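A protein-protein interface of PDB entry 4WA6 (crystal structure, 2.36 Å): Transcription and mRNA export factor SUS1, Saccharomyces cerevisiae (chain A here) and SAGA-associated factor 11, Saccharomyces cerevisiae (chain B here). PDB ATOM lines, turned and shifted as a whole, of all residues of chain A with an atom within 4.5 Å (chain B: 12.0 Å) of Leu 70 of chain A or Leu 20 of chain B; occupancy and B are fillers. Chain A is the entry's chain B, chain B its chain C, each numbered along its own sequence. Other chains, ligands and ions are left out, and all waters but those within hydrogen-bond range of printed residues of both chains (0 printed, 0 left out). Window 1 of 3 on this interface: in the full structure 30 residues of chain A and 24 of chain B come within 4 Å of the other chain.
OE2 of Glu 66 of chain A lies within hydrogen-bond range of NE2 of Gln 25 of chain B (2.9 Å).
Leu 70 of chain A touches two residues of chain B. Of chain A, only Leu 33, Leu 70, Val 73 and Arg 78 come within 4 Å of Leu 20 of chain B. No residue of chain B comes within 4 Å of Pro 67 of chain A. Ala 69 of chain A touches just one residue of chain B: Ile 24 (3.6 Å). No residue of chain B comes within 4 Å of Met 72 of chain A. Of chain B, only Leu 20 comes within 4 Å of Arg 78 of chain A. Of the printed residues of chain B, Leu 33 of chain A touches Leu 20 (3.9 Å) and Leu 23 (3.7 Å). Printed residues of chain A within 4 Å of Thr 21 of chain B: Glu 66 (3.4 Å). Printed residues of chain A within 4 Å of Leu 19 of chain B: Leu 29 (3.8 Å). Of the printed residues of chain B, Leu 29 of chain A touches Leu 19 (3.8 Å). Printed residues of chain B within 4 Å of Glu 66 of chain A: Thr 21 and Gln 25. The nearest residue of chain B that does not touch Leu 70 of chain A is Asn 17 of chain B (4.2 Å). The nearest printed residue of chain A that does not touch Thr 21 of chain B is Leu 70 of chain A (4.4 Å).
Of the 21 printed residues of chain B, 6 touch a printed residue of chain A. Hydrophobic or aromatic side chains of chain B that line the printed part of chain A: Leu 19, Leu 20, Leu 23 and Ile 24.
NE2 of Gln 25 of chain B lies close to O of Thr 21 of chain B (3.3 Å). O of Asn 17 of chain B sits at hydrogen-bond distance from OG1 of Thr 21 of chain B (2.5 Å). The backbone carbonyl oxygen (O) of Asn 18 of chain B is in hydrogen-bond range of the side-chain hydroxyl (OG1) of Thr 21 of chain B.
Among the printed residues, pairs that only touch across the chains: Leu 29 of chain A with Leu 19 of chain B (3.8 Å), Leu 33 of chain A with Leu 20 of chain B (3.9 Å), Leu 33 of chain A with Leu 23 of chain B (3.7 Å), Glu 66 of chain A with Thr 21 of chain B (3.4 Å), Ala 69 of chain A with Ile 24 of chain B (3.6 Å), Leu 70 of chain A with Leu 20 of chain B (3.7 Å), Leu 70 of chain A with Ile 24 of chain B (3.7 Å), Val 73 of chain A with Leu 20 of chain B (3.9 Å) and Arg 78 of chain A with Leu 20 of chain B (3.96 Å).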
ATOM      1  N   LEU A  29      11.948  -2.718 -10.962  1.00  0.00           N
ATOM      2  CA  LEU A  29      12.110  -2.021  -9.721  1.00  0.00           C
ATOM      3  C   LEU A  29      10.784  -1.464  -9.272  1.00  0.00           C
ATOM      4  O   LEU A  29      10.417  -1.596  -8.100  1.00  0.00           O
ATOM      5  CB  LEU A  29      13.129  -0.866  -9.890  1.00  0.00           C
ATOM      6  CG  LEU A  29      13.247   0.035  -8.704  1.00  0.00           C
ATOM      7  CD1 LEU A  29      13.631  -0.686  -7.417  1.00  0.00           C
ATOM      8  CD2 LEU A  29      14.254   1.123  -8.992  1.00  0.00           C
ATOM      9  N   LEU A  33       8.598  -2.146  -5.955  1.00  0.00           N
ATOM     10  CA  LEU A  33       8.307  -1.096  -4.985  1.00  0.00           C
ATOM     11  C   LEU A  33       6.802  -0.939  -4.793  1.00  0.00           C
ATOM     12  O   LEU A  33       6.336  -0.762  -3.699  1.00  0.00           O
ATOM     13  CB  LEU A  33       8.927   0.221  -5.431  1.00  0.00           C
ATOM     14  CG  LEU A  33      10.448   0.151  -5.426  1.00  0.00           C
ATOM     15  CD1 LEU A  33      11.044   1.417  -5.977  1.00  0.00           C
ATOM     16  CD2 LEU A  33      10.997  -0.097  -4.036  1.00  0.00           C
ATOM     17  N   GLU A  66      13.632  11.969   1.472  1.00  0.00           N
ATOM     18  CA  GLU A  66      14.413  11.108   0.575  1.00  0.00           C
ATOM     19  C   GLU A  66      15.314  10.128   1.336  1.00  0.00           C
ATOM     20  O   GLU A  66      15.258   8.940   1.095  1.00  0.00           O
ATOM     21  CB  GLU A  66      15.248  11.983  -0.392  1.00  0.00           C
ATOM     22  CG  GLU A  66      15.997  11.208  -1.473  1.00  0.00           C
ATOM     23  CD  GLU A  66      16.687  12.121  -2.465  1.00  0.00           C
ATOM     24  OE1 GLU A  66      17.692  12.777  -2.121  1.00  0.00           O
ATOM     25  OE2 GLU A  66      16.206  12.186  -3.607  1.00  0.00           O
ATOM     26  N   PRO A  67      16.113  10.615   2.287  1.00  0.00           N
ATOM     27  CA  PRO A  67      16.952   9.650   2.987  1.00  0.00           C
ATOM     28  C   PRO A  67      16.168   8.480   3.605  1.00  0.00           C
ATOM     29  O   PRO A  67      16.628   7.343   3.613  1.00  0.00           O
ATOM     30  CB  PRO A  67      17.617  10.490   4.111  1.00  0.00           C
ATOM     31  CG  PRO A  67      17.329  11.924   3.790  1.00  0.00           C
ATOM     32  CD  PRO A  67      16.127  11.950   2.904  1.00  0.00           C
ATOM     33  N   LYS A  68      14.990   8.789   4.147  1.00  0.00           N
ATOM     34  CA  LYS A  68      14.167   7.797   4.783  1.00  0.00           C
ATOM     35  C   LYS A  68      13.551   6.908   3.726  1.00  0.00           C
ATOM     36  O   LYS A  68      13.497   5.706   3.905  1.00  0.00           O
ATOM     37  CB  LYS A  68      13.088   8.454   5.604  1.00  0.00           C
ATOM     38  CG  LYS A  68      12.091   7.485   6.201  1.00  0.00           C
ATOM     39  CD  LYS A  68      12.686   6.732   7.374  1.00  0.00           C
ATOM     40  CE  LYS A  68      11.686   5.748   7.959  1.00  0.00           C
ATOM     41  NZ  LYS A  68      12.368   4.920   8.969  1.00  0.00           N
ATOM     42  N   ALA A  69      13.126   7.502   2.621  1.00  0.00           N
ATOM     43  CA  ALA A  69      12.571   6.751   1.538  1.00  0.00           C
ATOM     44  C   ALA A  69      13.624   5.770   1.004  1.00  0.00           C
ATOM     45  O   ALA A  69      13.315   4.618   0.743  1.00  0.00           O
ATOM     46  CB  ALA A  69      12.079   7.689   0.455  1.00  0.00           C
ATOM     47  N   LEU A  70      14.853   6.226   0.866  1.00  0.00           N
ATOM     48  CA  LEU A  70      15.962   5.335   0.517  1.00  0.00           C
ATOM     49  C   LEU A  70      16.136   4.123   1.467  1.00  0.00           C
ATOM     50  O   LEU A  70      16.210   2.978   1.018  1.00  0.00           O
ATOM     51  CB  LEU A  70      17.281   6.102   0.357  1.00  0.00           C
ATOM     52  CG  LEU A  70      17.301   7.020  -0.854  1.00  0.00           C
ATOM     53  CD1 LEU A  70      18.556   7.867  -0.767  1.00  0.00           C
ATOM     54  CD2 LEU A  70      17.198   6.337  -2.237  1.00  0.00           C
ATOM     55  N   GLU A  71      16.166   4.362   2.763  1.00  0.00           N
ATOM     56  CA  GLU A  71      16.273   3.256   3.721  1.00  0.00           C
ATOM     57  C   GLU A  71      15.073   2.305   3.771  1.00  0.00           C
ATOM     58  O   GLU A  71      15.190   1.200   4.248  1.00  0.00           O
ATOM     59  CB  GLU A  71      16.490   3.822   5.124  1.00  0.00           C
ATOM     60  CG  GLU A  71      17.833   4.510   5.276  1.00  0.00           C
ATOM     61  CD  GLU A  71      17.927   5.276   6.569  1.00  0.00           C
ATOM     62  OE1 GLU A  71      17.210   4.877   7.519  1.00  0.00           O
ATOM     63  OE2 GLU A  71      18.715   6.258   6.630  1.00  0.00           O
ATOM     64  N   MET A  72      13.916   2.757   3.334  1.00  0.00           N
ATOM     65  CA  MET A  72      12.703   1.960   3.408  1.00  0.00           C
ATOM     66  C   MET A  72      12.653   0.842   2.338  1.00  0.00           C
ATOM     67  O   MET A  72      11.900  -0.106   2.474  1.00  0.00           O
ATOM     68  CB  MET A  72      11.488   2.856   3.226  1.00  0.00           C
ATOM     69  CG  MET A  72      11.044   3.497   4.497  1.00  0.00           C
ATOM     70  SD  MET A  72       9.797   4.738   4.136  1.00  0.00           S
ATOM     71  CE  MET A  72       8.602   4.099   5.293  1.00  0.00           C
ATOM     72  N   VAL A  73      13.448   0.957   1.288  1.00  0.00           N
ATOM     73  CA  VAL A  73      13.472  -0.052   0.221  1.00  0.00           C
ATOM     74  C   VAL A  73      13.886  -1.367   0.827  1.00  0.00           C
ATOM     75  O   VAL A  73      14.878  -1.423   1.524  1.00  0.00           O
ATOM     76  CB  VAL A  73      14.477   0.354  -0.877  1.00  0.00           C
ATOM     77  CG1 VAL A  73      14.615  -0.727  -1.963  1.00  0.00           C
ATOM     78  CG2 VAL A  73      14.049   1.681  -1.496  1.00  0.00           C
ATOM     79  N   ARG A  78      16.387  -4.323  -3.220  1.00  0.00           N
ATOM     80  CA  ARG A  78      17.693  -3.735  -3.464  1.00  0.00           C
ATOM     81  C   ARG A  78      18.661  -4.744  -4.051  1.00  0.00           C
ATOM     82  O   ARG A  78      19.235  -4.475  -5.072  1.00  0.00           O
ATOM     83  CB  ARG A  78      18.263  -3.161  -2.159  1.00  0.00           C
ATOM     84  CG  ARG A  78      19.682  -2.618  -2.245  1.00  0.00           C
ATOM     85  CD  ARG A  78      19.994  -1.687  -1.070  1.00  0.00           C
ATOM     86  NE  ARG A  78      19.764  -0.258  -1.379  1.00  0.00           N
ATOM     87  CZ  ARG A  78      18.961   0.580  -0.710  1.00  0.00           C
ATOM     88  NH1 ARG A  78      18.252   0.180   0.354  1.00  0.00           N
ATOM     89  NH2 ARG A  78      18.865   1.851  -1.116  1.00  0.00           N
ATOM     90  N   SER B  10      30.323   0.379  -8.136  1.00  0.00           N
ATOM     91  CA  SER B  10      30.054   1.774  -8.011  1.00  0.00           C
ATOM     92  C   SER B  10      29.014   2.184  -9.043  1.00  0.00           C
ATOM     93  O   SER B  10      28.067   2.857  -8.678  1.00  0.00           O
ATOM     94  CB  SER B  10      31.326   2.595  -8.127  1.00  0.00           C
ATOM     95  OG  SER B  10      31.675   2.781  -9.483  1.00  0.00           O
ATOM     96  N   ILE B  11      29.154   1.740 -10.296  1.00  0.00           N
ATOM     97  CA  ILE B  11      28.201   2.084 -11.366  1.00  0.00           C
ATOM     98  C   ILE B  11      26.812   1.508 -11.136  1.00  0.00           C
ATOM     99  O   ILE B  11      25.818   2.191 -11.314  1.00  0.00           O
ATOM    100  CB  ILE B  11      28.686   1.624 -12.759  1.00  0.00           C
ATOM    101  CG1 ILE B  11      29.953   2.338 -13.165  1.00  0.00           C
ATOM    102  CG2 ILE B  11      27.640   1.842 -13.838  1.00  0.00           C
ATOM    103  CD1 ILE B  11      29.770   3.777 -13.508  1.00  0.00           C
ATOM    104  N   SER B  12      26.733   0.247 -10.761  1.00  0.00           N
ATOM    105  CA  SER B  12      25.438  -0.343 -10.395  1.00  0.00           C
ATOM    106  C   SER B  12      24.690   0.470  -9.369  1.00  0.00           C
ATOM    107  O   SER B  12      23.493   0.700  -9.481  1.00  0.00           O
ATOM    108  CB  SER B  12      25.649  -1.698  -9.763  1.00  0.00           C
ATOM    109  OG  SER B  12      26.693  -2.352 -10.430  1.00  0.00           O
ATOM    110  N   ASN B  13      25.402   0.828  -8.307  1.00  0.00           N
ATOM    111  CA  ASN B  13      24.815   1.556  -7.210  1.00  0.00           C
ATOM    112  C   ASN B  13      24.431   2.957  -7.657  1.00  0.00           C
ATOM    113  O   ASN B  13      23.402   3.485  -7.197  1.00  0.00           O
ATOM    114  CB  ASN B  13      25.796   1.633  -6.051  1.00  0.00           C
ATOM    115  CG  ASN B  13      25.903   0.337  -5.289  1.00  0.00           C
ATOM    116  OD1 ASN B  13      24.923  -0.238  -4.825  1.00  0.00           O
ATOM    117  ND2 ASN B  13      27.094  -0.110  -5.130  1.00  0.00           N
ATOM    118  N   GLY B  14      25.239   3.528  -8.561  1.00  0.00           N
ATOM    119  CA  GLY B  14      24.934   4.805  -9.146  1.00  0.00           C
ATOM    120  C   GLY B  14      23.600   4.724  -9.853  1.00  0.00           C
ATOM    121  O   GLY B  14      22.727   5.579  -9.637  1.00  0.00           O
ATOM    122  N   ILE B  15      23.406   3.671 -10.650  1.00  0.00           N
ATOM    123  CA  ILE B  15      22.209   3.547 -11.414  1.00  0.00           C
ATOM    124  C   ILE B  15      20.984   3.366 -10.533  1.00  0.00           C
ATOM    125  O   ILE B  15      19.974   4.069 -10.686  1.00  0.00           O
ATOM    126  CB  ILE B  15      22.331   2.411 -12.420  1.00  0.00           C
ATOM    127  CG1 ILE B  15      23.267   2.853 -13.519  1.00  0.00           C
ATOM    128  CG2 ILE B  15      20.976   2.038 -13.009  1.00  0.00           C
ATOM    129  CD1 ILE B  15      23.868   1.695 -14.263  1.00  0.00           C
ATOM    130  N   LEU B  16      21.056   2.441  -9.597  1.00  0.00           N
ATOM    131  CA  LEU B  16      19.949   2.233  -8.648  1.00  0.00           C
ATOM    132  C   LEU B  16      19.541   3.520  -7.913  1.00  0.00           C
ATOM    133  O   LEU B  16      18.343   3.855  -7.790  1.00  0.00           O
ATOM    134  CB  LEU B  16      20.348   1.180  -7.636  1.00  0.00           C
ATOM    135  CG  LEU B  16      19.319   0.908  -6.562  1.00  0.00           C
ATOM    136  CD1 LEU B  16      17.980   0.649  -7.191  1.00  0.00           C
ATOM    137  CD2 LEU B  16      19.739  -0.300  -5.770  1.00  0.00           C
ATOM    138  N   ASN B  17      20.544   4.271  -7.481  1.00  0.00           N
ATOM    139  CA  ASN B  17      20.301   5.481  -6.707  1.00  0.00           C
ATOM    140  C   ASN B  17      19.679   6.576  -7.591  1.00  0.00           C
ATOM    141  O   ASN B  17      18.796   7.326  -7.155  1.00  0.00           O
ATOM    142  CB  ASN B  17      21.609   5.945  -6.071  1.00  0.00           C
ATOM    143  CG  ASN B  17      21.425   7.195  -5.239  1.00  0.00           C
ATOM    144  OD1 ASN B  17      21.002   7.123  -4.097  1.00  0.00           O
ATOM    145  ND2 ASN B  17      21.735   8.345  -5.798  1.00  0.00           N
ATOM    146  N   ASN B  18      20.143   6.649  -8.831  1.00  0.00           N
ATOM    147  CA  ASN B  18      19.522   7.481  -9.846  1.00  0.00           C
ATOM    148  C   ASN B  18      18.055   7.122  -9.994  1.00  0.00           C
ATOM    149  O   ASN B  18      17.231   8.007  -9.920  1.00  0.00           O
ATOM    150  CB  ASN B  18      20.208   7.365 -11.222  1.00  0.00           C
ATOM    151  CG  ASN B  18      21.500   8.198 -11.326  1.00  0.00           C
ATOM    152  OD1 ASN B  18      22.025   8.675 -10.375  1.00  0.00           O
ATOM    153  ND2 ASN B  18      22.017   8.315 -12.520  1.00  0.00           N
ATOM    154  N   LEU B  19      17.744   5.827 -10.143  1.00  0.00           N
ATOM    155  CA  LEU B  19      16.340   5.412 -10.307  1.00  0.00           C
ATOM    156  C   LEU B  19      15.562   5.716  -9.051  1.00  0.00           C
ATOM    157  O   LEU B  19      14.512   6.346  -9.141  1.00  0.00           O
ATOM    158  CB  LEU B  19      16.172   3.935 -10.633  1.00  0.00           C
ATOM    159  CG  LEU B  19      16.753   3.401 -11.939  1.00  0.00           C
ATOM    160  CD1 LEU B  19      16.812   1.883 -11.963  1.00  0.00           C
ATOM    161  CD2 LEU B  19      15.913   3.902 -13.063  1.00  0.00           C
ATOM    162  N   LEU B  20      16.059   5.329  -7.881  1.00  0.00           N
ATOM    163  CA  LEU B  20      15.275   5.568  -6.641  1.00  0.00           C
ATOM    164  C   LEU B  20      14.994   7.031  -6.381  1.00  0.00           C
ATOM    165  O   LEU B  20      13.897   7.373  -6.010  1.00  0.00           O
ATOM    166  CB  LEU B  20      15.970   4.956  -5.435  1.00  0.00           C
ATOM    167  CG  LEU B  20      15.919   3.433  -5.440  1.00  0.00           C
ATOM    168  CD1 LEU B  20      16.895   2.829  -4.414  1.00  0.00           C
ATOM    169  CD2 LEU B  20      14.455   3.043  -5.170  1.00  0.00           C
ATOM    170  N   THR B  21      15.992   7.887  -6.602  1.00  0.00           N
ATOM    171  CA  THR B  21      15.871   9.314  -6.247  1.00  0.00           C
ATOM    172  C   THR B  21      14.968  10.025  -7.253  1.00  0.00           C
ATOM    173  O   THR B  21      14.168  10.915  -6.898  1.00  0.00           O
ATOM    174  CB  THR B  21      17.234  10.043  -6.238  1.00  0.00           C
ATOM    175  OG1 THR B  21      17.958   9.684  -7.439  1.00  0.00           O
ATOM    176  CG2 THR B  21      18.012   9.673  -5.044  1.00  0.00           C
ATOM    177  N   THR B  22      15.109   9.642  -8.511  1.00  0.00           N
ATOM    178  CA  THR B  22      14.203  10.134  -9.504  1.00  0.00           C
ATOM    179  C   THR B  22      12.742   9.819  -9.094  1.00  0.00           C
ATOM    180  O   THR B  22      11.875  10.763  -8.993  1.00  0.00           O
ATOM    181  CB  THR B  22      14.586   9.583 -10.867  1.00  0.00           C
ATOM    182  OG1 THR B  22      15.914  10.058 -11.177  1.00  0.00           O
ATOM    183  CG2 THR B  22      13.564  10.001 -11.919  1.00  0.00           C
ATOM    184  N   LEU B  23      12.497   8.540  -8.782  1.00  0.00           N
ATOM    185  CA  LEU B  23      11.157   8.083  -8.342  1.00  0.00           C
ATOM    186  C   LEU B  23      10.696   8.836  -7.084  1.00  0.00           C
ATOM    187  O   LEU B  23       9.590   9.421  -7.085  1.00  0.00           O
ATOM    188  CB  LEU B  23      11.126   6.581  -8.095  1.00  0.00           C
ATOM    189  CG  LEU B  23       9.746   6.005  -7.700  1.00  0.00           C
ATOM    190  CD1 LEU B  23       8.577   6.368  -8.645  1.00  0.00           C
ATOM    191  CD2 LEU B  23       9.899   4.494  -7.586  1.00  0.00           C
ATOM    192  N   ILE B  24      11.553   8.891  -6.054  1.00  0.00           N
ATOM    193  CA  ILE B  24      11.201   9.609  -4.838  1.00  0.00           C
ATOM    194  C   ILE B  24      10.892  11.088  -5.083  1.00  0.00           C
ATOM    195  O   ILE B  24       9.980  11.631  -4.503  1.00  0.00           O
ATOM    196  CB  ILE B  24      12.326   9.573  -3.808  1.00  0.00           C
ATOM    197  CG1 ILE B  24      12.505   8.165  -3.309  1.00  0.00           C
ATOM    198  CG2 ILE B  24      12.023  10.506  -2.596  1.00  0.00           C
ATOM    199  CD1 ILE B  24      13.855   7.910  -2.661  1.00  0.00           C
ATOM    200  N   GLN B  25      11.689  11.742  -5.903  1.00  0.00           N
ATOM    201  CA  GLN B  25      11.483  13.133  -6.198  1.00  0.00           C
ATOM    202  C   GLN B  25      10.183  13.404  -6.882  1.00  0.00           C
ATOM    203  O   GLN B  25       9.550  14.480  -6.716  1.00  0.00           O
ATOM    204  CB  GLN B  25      12.651  13.696  -7.006  1.00  0.00           C
ATOM    205  CG  GLN B  25      13.863  13.888  -6.108  1.00  0.00           C
ATOM    206  CD  GLN B  25      15.186  14.000  -6.838  1.00  0.00           C
ATOM    207  OE1 GLN B  25      15.280  14.650  -7.863  1.00  0.00           O
ATOM    208  NE2 GLN B  25      16.228  13.393  -6.274  1.00  0.00           N
ATOM    209  N   ASP B  26       9.801  12.455  -7.667  1.00  0.00           N
ATOM    210  CA  ASP B  26       8.597  12.553  -8.469  1.00  0.00           C
ATOM    211  C   ASP B  26       7.402  12.407  -7.535  1.00  0.00           C
ATOM    212  O   ASP B  26       6.500  13.190  -7.596  1.00  0.00           O
ATOM    213  CB  ASP B  26       8.575  11.423  -9.512  1.00  0.00           C
ATOM    214  CG  ASP B  26       7.324  11.447 -10.398  1.00  0.00           C
ATOM    215  OD1 ASP B  26       6.597  12.495 -10.562  1.00  0.00           O
ATOM    216  OD2 ASP B  26       7.039  10.371 -10.942  1.00  0.00           O
ATOM    217  N   ILE B  27       7.396  11.369  -6.700  1.00  0.00           N
ATOM    218  CA  ILE B  27       6.323  11.178  -5.746  1.00  0.00           C
ATOM    219  C   ILE B  27       6.239  12.415  -4.838  1.00  0.00           C
ATOM    220  O   ILE B  27       5.127  12.887  -4.538  1.00  0.00           O
ATOM    221  CB  ILE B  27       6.554   9.900  -4.911  1.00  0.00           C
ATOM    222  CG1 ILE B  27       6.352   8.623  -5.745  1.00  0.00           C
ATOM    223  CG2 ILE B  27       5.688   9.812  -3.675  1.00  0.00           C
ATOM    224  CD1 ILE B  27       7.066   7.461  -5.086  1.00  0.00           C
ATOM    225  N   VAL B  28       7.383  12.970  -4.421  1.00  0.00           N
ATOM    226  CA  VAL B  28       7.331  14.105  -3.544  1.00  0.00           C
ATOM    227  C   VAL B  28       6.780  15.369  -4.222  1.00  0.00           C
ATOM    228  O   VAL B  28       5.973  16.105  -3.632  1.00  0.00           O
ATOM    229  CB  VAL B  28       8.639  14.306  -2.788  1.00  0.00           C
ATOM    230  CG1 VAL B  28       8.573  15.530  -1.908  1.00  0.00           C
ATOM    231  CG2 VAL B  28       8.857  13.133  -1.848  1.00  0.00           C
ATOM    232  N   ALA B  29       7.154  15.583  -5.472  1.00  0.00           N
ATOM    233  CA  ALA B  29       6.612  16.698  -6.240  1.00  0.00           C
ATOM    234  C   ALA B  29       5.089  16.625  -6.344  1.00  0.00           C
ATOM    235  O   ALA B  29       4.383  17.620  -6.213  1.00  0.00           O
ATOM    236  CB  ALA B  29       7.249  16.758  -7.628  1.00  0.00           C
ATOM    237  N   ARG B  30       4.567  15.440  -6.593  1.00  0.00           N
ATOM    238  CA  ARG B  30       3.140  15.322  -6.702  1.00  0.00           C
ATOM    239  C   ARG B  30       2.406  15.605  -5.422  1.00  0.00           C
ATOM    240  O   ARG B  30       1.480  16.398  -5.419  1.00  0.00           O
ATOM    241  CB  ARG B  30       2.804  13.969  -7.232  1.00  0.00           C
ATOM    242  CG  ARG B  30       3.326  13.855  -8.623  1.00  0.00           C
ATOM    243  CD  ARG B  30       2.874  12.560  -9.136  1.00  0.00           C
ATOM    244  NE  ARG B  30       3.769  12.025 -10.113  1.00  0.00           N
ATOM    245  CZ  ARG B  30       3.399  11.639 -11.327  1.00  0.00           C
ATOM    246  NH1 ARG B  30       2.147  11.817 -11.712  1.00  0.00           N
ATOM    247  NH2 ARG B  30       4.291  11.108 -12.168  1.00  0.00           N
